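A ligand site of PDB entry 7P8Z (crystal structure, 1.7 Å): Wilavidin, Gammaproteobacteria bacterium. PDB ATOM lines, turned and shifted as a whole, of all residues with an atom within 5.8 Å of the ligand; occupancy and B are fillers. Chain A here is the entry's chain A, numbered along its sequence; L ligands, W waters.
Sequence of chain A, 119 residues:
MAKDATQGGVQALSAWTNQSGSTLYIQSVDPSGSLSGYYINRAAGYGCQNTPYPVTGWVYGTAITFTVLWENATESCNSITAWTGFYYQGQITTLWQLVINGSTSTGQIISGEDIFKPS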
ATOM      1  N   ASN A  18     -11.453  -8.602 -16.345  1.00  0.00           N
ATOM      2  CA  ASN A  18     -11.276  -7.858 -15.071  1.00  0.00           C
ATOM      3  C   ASN A  18     -10.838  -6.423 -15.400  1.00  0.00           C
ATOM      4  O   ASN A  18     -10.799  -5.992 -16.589  1.00  0.00           O
ATOM      5  CB  ASN A  18     -10.447  -8.644 -14.061  1.00  0.00           C
ATOM      6  CG  ASN A  18      -8.996  -8.813 -14.433  1.00  0.00           C
ATOM      7  OD1 ASN A  18      -8.315  -9.747 -13.951  1.00  0.00           O
ATOM      8  ND2 ASN A  18      -8.528  -7.984 -15.344  1.00  0.00           N
ATOM      9  N   SER A  20      -8.031  -5.089 -15.030  1.00  0.00           N
ATOM     10  CA  SER A  20      -6.686  -5.094 -15.648  1.00  0.00           C
ATOM     11  C   SER A  20      -6.758  -5.490 -17.133  1.00  0.00           C
ATOM     12  O   SER A  20      -5.694  -5.315 -17.811  1.00  0.00           O
ATOM     13  CB  SER A  20      -5.776  -6.005 -14.873  1.00  0.00           C
ATOM     14  OG  SER A  20      -5.705  -5.585 -13.522  1.00  0.00           O
ATOM     15  N   SER A  22      -7.602  -8.572 -18.213  1.00  0.00           N
ATOM     16  CA  SER A  22      -7.408 -10.036 -18.329  1.00  0.00           C
ATOM     17  C   SER A  22      -8.766 -10.698 -18.509  1.00  0.00           C
ATOM     18  O   SER A  22      -9.779 -10.169 -17.985  1.00  0.00           O
ATOM     19  CB  SER A  22      -6.657 -10.607 -17.127  1.00  0.00           C
ATOM     20  OG  SER A  22      -5.483  -9.825 -16.904  1.00  0.00           O
ATOM     21  N   TYR A  39      -7.450 -18.712 -19.687  1.00  0.00           N
ATOM     22  CA  TYR A  39      -7.295 -17.372 -19.086  1.00  0.00           C
ATOM     23  C   TYR A  39      -6.216 -16.677 -19.902  1.00  0.00           C
ATOM     24  O   TYR A  39      -5.149 -17.252 -20.201  1.00  0.00           O
ATOM     25  CB  TYR A  39      -7.005 -17.500 -17.598  1.00  0.00           C
ATOM     26  CG  TYR A  39      -7.034 -16.215 -16.837  1.00  0.00           C
ATOM     27  CD1 TYR A  39      -5.958 -15.334 -16.853  1.00  0.00           C
ATOM     28  CD2 TYR A  39      -8.145 -15.890 -16.084  1.00  0.00           C
ATOM     29  CE1 TYR A  39      -6.022 -14.155 -16.138  1.00  0.00           C
ATOM     30  CE2 TYR A  39      -8.191 -14.742 -15.346  1.00  0.00           C
ATOM     31  CZ  TYR A  39      -7.112 -13.890 -15.333  1.00  0.00           C
ATOM     32  OH  TYR A  39      -7.229 -12.703 -14.642  1.00  0.00           O
ATOM     33  N   ASN A  41      -4.017 -13.380 -19.546  1.00  0.00           N
ATOM     34  CA  ASN A  41      -3.530 -12.332 -18.633  1.00  0.00           C
ATOM     35  C   ASN A  41      -3.134 -11.075 -19.436  1.00  0.00           C
ATOM     36  O   ASN A  41      -2.366 -11.162 -20.373  1.00  0.00           O
ATOM     37  CB  ASN A  41      -2.381 -12.903 -17.844  1.00  0.00           C
ATOM     38  CG  ASN A  41      -1.719 -11.857 -16.995  1.00  0.00           C
ATOM     39  OD1 ASN A  41      -2.384 -10.994 -16.397  1.00  0.00           O
ATOM     40  ND2 ASN A  41      -0.436 -11.952 -16.897  1.00  0.00           N
ATOM     41  N   ARG A  42      -3.661  -9.908 -19.082  1.00  0.00           N
ATOM     42  CA  ARG A  42      -3.287  -8.640 -19.755  1.00  0.00           C
ATOM     43  C   ARG A  42      -2.937  -7.597 -18.684  1.00  0.00           C
ATOM     44  O   ARG A  42      -2.853  -6.362 -18.995  1.00  0.00           O
ATOM     45  CB  ARG A  42      -4.432  -8.284 -20.701  1.00  0.00           C
ATOM     46  CG  ARG A  42      -4.732  -9.333 -21.769  1.00  0.00           C
ATOM     47  CD  ARG A  42      -5.595  -8.695 -22.845  1.00  0.00           C
ATOM     48  NE  ARG A  42      -6.245  -9.724 -23.653  1.00  0.00           N
ATOM     49  CZ  ARG A  42      -7.357 -10.413 -23.334  1.00  0.00           C
ATOM     50  NH1 ARG A  42      -8.049 -10.159 -22.230  1.00  0.00           N
ATOM     51  NH2 ARG A  42      -7.780 -11.355 -24.173  1.00  0.00           N
ATOM     52  N   ALA A  43      -2.521  -8.099 -17.527  1.00  0.00           N
ATOM     53  CA  ALA A  43      -2.220  -7.240 -16.347  1.00  0.00           C
ATOM     54  C   ALA A  43      -0.804  -6.683 -16.497  1.00  0.00           C
ATOM     55  O   ALA A  43       0.136  -7.545 -16.574  1.00  0.00           O
ATOM     56  CB  ALA A  43      -2.358  -8.000 -15.078  1.00  0.00           C
ATOM     57  N   TYR A  46       3.083  -7.942 -15.175  1.00  0.00           N
ATOM     58  CA  TYR A  46       3.172  -9.411 -14.955  1.00  0.00           C
ATOM     59  C   TYR A  46       3.710 -10.046 -16.212  1.00  0.00           C
ATOM     60  O   TYR A  46       3.597  -9.499 -17.339  1.00  0.00           O
ATOM     61  CB  TYR A  46       1.830 -10.018 -14.542  1.00  0.00           C
ATOM     62  CG  TYR A  46       1.325  -9.535 -13.196  1.00  0.00           C
ATOM     63  CD1 TYR A  46       0.577  -8.372 -13.085  1.00  0.00           C
ATOM     64  CD2 TYR A  46       1.569 -10.247 -12.028  1.00  0.00           C
ATOM     65  CE1 TYR A  46       0.067  -7.943 -11.865  1.00  0.00           C
ATOM     66  CE2 TYR A  46       1.045  -9.832 -10.807  1.00  0.00           C
ATOM     67  CZ  TYR A  46       0.288  -8.674 -10.718  1.00  0.00           C
ATOM     68  OH  TYR A  46      -0.227  -8.268  -9.504  1.00  0.00           O
ATOM     69  N   GLY A  47       4.174 -11.265 -16.049  1.00  0.00           N
ATOM     70  CA  GLY A  47       4.592 -12.045 -17.214  1.00  0.00           C
ATOM     71  C   GLY A  47       3.368 -12.761 -17.782  1.00  0.00           C
ATOM     72  O   GLY A  47       2.204 -12.489 -17.325  1.00  0.00           O
ATOM     73  N   CYS A  48       3.623 -13.631 -18.752  1.00  0.00           N
ATOM     74  CA  CYS A  48       2.635 -14.553 -19.276  1.00  0.00           C
ATOM     75  C   CYS A  48       1.409 -13.735 -19.659  1.00  0.00           C
ATOM     76  O   CYS A  48       0.294 -14.089 -19.287  1.00  0.00           O
ATOM     77  CB  CYS A  48       2.294 -15.624 -18.253  1.00  0.00           C
ATOM     78  SG  CYS A  48       3.722 -16.720 -18.017  1.00  0.00           S
ATOM     79  N   TRP A  70       0.534 -20.989 -14.747  1.00  0.00           N
ATOM     80  CA  TRP A  70       1.205 -20.036 -15.693  1.00  0.00           C
ATOM     81  C   TRP A  70       2.305 -20.764 -16.453  1.00  0.00           C
ATOM     82  O   TRP A  70       3.454 -20.389 -16.367  1.00  0.00           O
ATOM     83  CB  TRP A  70       1.723 -18.802 -14.968  1.00  0.00           C
ATOM     84  CG  TRP A  70       0.605 -18.113 -14.244  1.00  0.00           C
ATOM     85  CD1 TRP A  70       0.373 -18.041 -12.910  1.00  0.00           C
ATOM     86  CD2 TRP A  70      -0.429 -17.372 -14.879  1.00  0.00           C
ATOM     87  NE1 TRP A  70      -0.706 -17.249 -12.648  1.00  0.00           N
ATOM     88  CE2 TRP A  70      -1.245 -16.864 -13.837  1.00  0.00           C
ATOM     89  CE3 TRP A  70      -0.749 -17.102 -16.209  1.00  0.00           C
ATOM     90  CZ2 TRP A  70      -2.344 -16.107 -14.089  1.00  0.00           C
ATOM     91  CZ3 TRP A  70      -1.903 -16.403 -16.460  1.00  0.00           C
ATOM     92  CH2 TRP A  70      -2.634 -15.893 -15.408  1.00  0.00           C
ATOM     93  N   CYS A  77       5.809 -18.899 -16.388  1.00  0.00           N
ATOM     94  CA  CYS A  77       6.199 -18.002 -15.260  1.00  0.00           C
ATOM     95  C   CYS A  77       6.325 -18.776 -13.935  1.00  0.00           C
ATOM     96  O   CYS A  77       6.497 -18.116 -12.905  1.00  0.00           O
ATOM     97  CB  CYS A  77       5.252 -16.828 -15.104  1.00  0.00           C
ATOM     98  SG  CYS A  77       5.143 -15.771 -16.581  1.00  0.00           S
ATOM     99  N   SER A  79       4.640 -20.325 -11.780  1.00  0.00           N
ATOM    100  CA  SER A  79       3.739 -19.805 -10.719  1.00  0.00           C
ATOM    101  C   SER A  79       2.340 -20.374 -10.933  1.00  0.00           C
ATOM    102  O   SER A  79       1.984 -20.822 -12.102  1.00  0.00           O
ATOM    103  CB  SER A  79       3.819 -18.311 -10.693  1.00  0.00           C
ATOM    104  OG  SER A  79       3.529 -17.724 -11.948  1.00  0.00           O
ATOM    105  N   THR A  81      -1.926 -19.139  -9.915  1.00  0.00           N
ATOM    106  CA  THR A  81      -2.843 -18.214  -9.213  1.00  0.00           C
ATOM    107  C   THR A  81      -4.134 -18.969  -8.921  1.00  0.00           C
ATOM    108  O   THR A  81      -4.604 -19.743  -9.792  1.00  0.00           O
ATOM    109  CB  THR A  81      -3.119 -16.913  -9.976  1.00  0.00           C
ATOM    110  OG1 THR A  81      -1.892 -16.234 -10.223  1.00  0.00           O
ATOM    111  CG2 THR A  81      -4.082 -15.985  -9.233  1.00  0.00           C
ATOM    112  N   TRP A  83      -8.018 -17.909  -7.588  1.00  0.00           N
ATOM    113  CA  TRP A  83      -9.065 -16.912  -7.295  1.00  0.00           C
ATOM    114  C   TRP A  83     -10.212 -17.543  -6.512  1.00  0.00           C
ATOM    115  O   TRP A  83     -10.682 -18.594  -6.890  1.00  0.00           O
ATOM    116  CB  TRP A  83      -9.679 -16.336  -8.592  1.00  0.00           C
ATOM    117  CG  TRP A  83      -8.798 -15.425  -9.329  1.00  0.00           C
ATOM    118  CD1 TRP A  83      -8.904 -14.088  -9.404  1.00  0.00           C
ATOM    119  CD2 TRP A  83      -7.810 -15.819 -10.295  1.00  0.00           C
ATOM    120  NE1 TRP A  83      -8.016 -13.588 -10.322  1.00  0.00           N
ATOM    121  CE2 TRP A  83      -7.337 -14.629 -10.904  1.00  0.00           C
ATOM    122  CE3 TRP A  83      -7.274 -17.049 -10.673  1.00  0.00           C
ATOM    123  CZ2 TRP A  83      -6.366 -14.662 -11.891  1.00  0.00           C
ATOM    124  CZ3 TRP A  83      -6.355 -17.103 -11.678  1.00  0.00           C
ATOM    125  CH2 TRP A  83      -5.883 -15.898 -12.259  1.00  0.00           C
ATOM    126  N   TRP A  96      -7.486 -13.064  -5.003  1.00  0.00           N
ATOM    127  CA  TRP A  96      -6.550 -14.059  -5.577  1.00  0.00           C
ATOM    128  C   TRP A  96      -5.274 -14.131  -4.776  1.00  0.00           C
ATOM    129  O   TRP A  96      -4.921 -13.129  -4.191  1.00  0.00           O
ATOM    130  CB  TRP A  96      -6.263 -13.803  -7.054  1.00  0.00           C
ATOM    131  CG  TRP A  96      -5.773 -12.442  -7.362  1.00  0.00           C
ATOM    132  CD1 TRP A  96      -6.495 -11.358  -7.797  1.00  0.00           C
ATOM    133  CD2 TRP A  96      -4.388 -12.045  -7.363  1.00  0.00           C
ATOM    134  NE1 TRP A  96      -5.654 -10.301  -8.040  1.00  0.00           N
ATOM    135  CE2 TRP A  96      -4.363 -10.689  -7.771  1.00  0.00           C
ATOM    136  CE3 TRP A  96      -3.181 -12.653  -6.985  1.00  0.00           C
ATOM    137  CZ2 TRP A  96      -3.183  -9.947  -7.791  1.00  0.00           C
ATOM    138  CZ3 TRP A  96      -2.018 -11.911  -7.093  1.00  0.00           C
ATOM    139  CH2 TRP A  96      -2.015 -10.589  -7.519  1.00  0.00           C
ATOM    140  N   LEU A  98      -1.199 -15.771  -5.547  1.00  0.00           N
ATOM    141  CA  LEU A  98      -0.227 -16.177  -6.567  1.00  0.00           C
ATOM    142  C   LEU A  98       0.968 -16.779  -5.844  1.00  0.00           C
ATOM    143  O   LEU A  98       1.591 -16.082  -4.991  1.00  0.00           O
ATOM    144  CB  LEU A  98       0.208 -14.985  -7.397  1.00  0.00           C
ATOM    145  CG  LEU A  98       1.306 -15.236  -8.437  1.00  0.00           C
ATOM    146  CD1 LEU A  98       1.040 -16.449  -9.255  1.00  0.00           C
ATOM    147  CD2 LEU A  98       1.399 -14.109  -9.406  1.00  0.00           C
ATOM    148  N   ILE A 100       4.736 -18.961  -6.331  1.00  0.00           N
ATOM    149  CA  ILE A 100       5.838 -19.242  -7.287  1.00  0.00           C
ATOM    150  C   ILE A 100       6.487 -20.546  -6.857  1.00  0.00           C
ATOM    151  O   ILE A 100       6.738 -20.726  -5.631  1.00  0.00           O
ATOM    152  CB  ILE A 100       6.832 -18.075  -7.268  1.00  0.00           C
ATOM    153  CG1 ILE A 100       6.056 -16.765  -7.327  1.00  0.00           C
ATOM    154  CG2 ILE A 100       7.812 -18.259  -8.416  1.00  0.00           C
ATOM    155  CD1 ILE A 100       6.898 -15.522  -7.236  1.00  0.00           C
ATOM    156  N   ASP A 114      -9.524  -8.994  -7.899  1.00  0.00           N
ATOM    157  CA  ASP A 114      -9.986  -8.784  -9.290  1.00  0.00           C
ATOM    158  C   ASP A 114     -11.517  -8.743  -9.339  1.00  0.00           C
ATOM    159  O   ASP A 114     -12.250  -9.703  -8.829  1.00  0.00           O
ATOM    160  CB  ASP A 114      -9.519  -9.908 -10.198  1.00  0.00           C
ATOM    161  CG  ASP A 114      -8.078  -9.808 -10.629  1.00  0.00           C
ATOM    162  OD1 ASP A 114      -7.456  -8.727 -10.486  1.00  0.00           O
ATOM    163  OD2 ASP A 114      -7.584 -10.848 -11.033  1.00  0.00           O
ATOM    164  N   PHE A 116     -14.480  -9.014 -12.267  1.00  0.00           N
ATOM    165  CA  PHE A 116     -14.729  -9.459 -13.655  1.00  0.00           C
ATOM    166  C   PHE A 116     -16.115  -9.042 -14.124  1.00  0.00           C
ATOM    167  O   PHE A 116     -17.076  -9.286 -13.372  1.00  0.00           O
ATOM    168  CB  PHE A 116     -14.582 -10.976 -13.747  1.00  0.00           C
ATOM    169  CG  PHE A 116     -13.190 -11.474 -13.479  1.00  0.00           C
ATOM    170  CD1 PHE A 116     -12.767 -11.718 -12.195  1.00  0.00           C
ATOM    171  CD2 PHE A 116     -12.314 -11.721 -14.531  1.00  0.00           C
ATOM    172  CE1 PHE A 116     -11.469 -12.154 -11.944  1.00  0.00           C
ATOM    173  CE2 PHE A 116     -11.030 -12.171 -14.279  1.00  0.00           C
ATOM    174  CZ  PHE A 116     -10.596 -12.358 -12.996  1.00  0.00           C
HETATM  175  C1  LIG L   1       3.205 -14.311 -13.188  1.00  0.00           C
HETATM  176  O1  LIG L   1       3.415 -13.167 -13.425  1.00  0.00           O
HETATM  177  O2  LIG L   1       3.708 -14.940 -12.190  1.00  0.00           O
HETATM  178  C2  LIG L   1       2.257 -14.857 -14.189  1.00  0.00           C
HETATM  179  C3  LIG L   1       0.913 -14.114 -14.348  1.00  0.00           C
HETATM  180  C4  LIG L   1       0.276 -13.620 -13.100  1.00  0.00           C
HETATM  181  C5  LIG L   1      -0.906 -12.690 -13.479  1.00  0.00           C
HETATM  182  C6  LIG L   1      -1.768 -12.178 -12.301  1.00  0.00           C
HETATM  183  S1  LIG L   1      -2.901 -13.473 -11.697  1.00  0.00           S
HETATM  184  C7  LIG L   1      -3.585 -12.289 -10.549  1.00  0.00           C
HETATM  185  C8  LIG L   1      -3.724 -10.981 -11.376  1.00  0.00           C
HETATM  186  N1  LIG L   1      -4.980 -10.914 -12.107  1.00  0.00           N
HETATM  187  C9  LIG L   1      -4.725 -10.802 -13.461  1.00  0.00           C
HETATM  188  O3  LIG L   1      -5.509 -10.523 -14.343  1.00  0.00           O
HETATM  189  N2  LIG L   1      -3.412 -10.921 -13.719  1.00  0.00           N
HETATM  190  C10 LIG L   1      -2.650 -10.949 -12.450  1.00  0.00           C
HETATM  191  O   HOH W   1      -5.109  -7.811 -11.741  1.00  0.00           O
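OH of Tyr 39 lies within hydrogen-bond range of O3 of the ligand, at 2.8 Å.
N1 of the ligand is in hydrogen-bond range of OD2 of Asp 114.
An oxygen (O3) of the ligand sits at hydrogen-bond distance from the side-chain hydroxyl (OG) of Ser 22, 2.7 Å away.
A nitrogen (N2) of the ligand is in hydrogen-bond range of the side-chain amide oxygen of Asn 41, 2.9 Å away.
The backbone NH (N) of Gly 47 sits at hydrogen-bond distance from an oxygen (O1) of the ligand, 3.3 Å away.
OG1 of Thr 81 lies close to S1 of the ligand, 3.3 Å away.
The side-chain hydroxyl (OG) of Ser 79 is in hydrogen-bond range of an oxygen (O2) of the ligand (2.8 Å).
The side-chain amide oxygen (OD1) of Asn 18 lies close to an oxygen (O3) of the ligand (2.9 Å).
The side-chain hydroxyl of Ser 22 lies within hydrogen-bond range of the backbone NH of Ala 43 (3.5 Å).
The side-chain hydroxyl (OH) of Tyr 39 sits at hydrogen-bond distance from the side-chain amide oxygen (OD1) of Asn 18.
The side-chain hydroxyl (OG) of Ser 79 sits at hydrogen-bond distance from the backbone carbonyl oxygen (O) of Cys 77 (3.1 Å).
The backbone NH (N) of Trp 70 lies within hydrogen-bond range of the backbone carbonyl oxygen (O) of Ser 79.
O of Gly 47 sits at hydrogen-bond distance from ND2 of Asn 41.
OD1 of Asp 114 lies within hydrogen-bond range of NE1 of Trp 96.
The backbone carbonyl oxygen of Trp 70 sits at hydrogen-bond distance from the backbone NH of Cys 77, 2.8 Å away.
OD1 of Asn 41 lies within hydrogen-bond range of OG of Ser 22, at 3.4 Å.
Residues that only touch the ligand: Trp 96 (3.3 Å), Ala 43 (3.4 Å), Trp 70 (3.5 Å), Trp 83 (3.7 Å), Tyr 46 (3.7 Å), Cys 77 (3.7 Å) and Leu 98 (3.7 Å).
Hydrophobic or aromatic side chains within 4 Å of the ligand: Tyr 39, Ala 43, Tyr 46, Trp 70, Trp 83, Trp 96 and Leu 98.
Water W1 lies within hydrogen-bond range of the side-chain carboxylate (OD1) of Asp 114 (2.8 Å), the side-chain hydroxyl (OG) of Ser 20 (2.9 Å) and a nitrogen (N1) of the ligand (3.1 Å).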
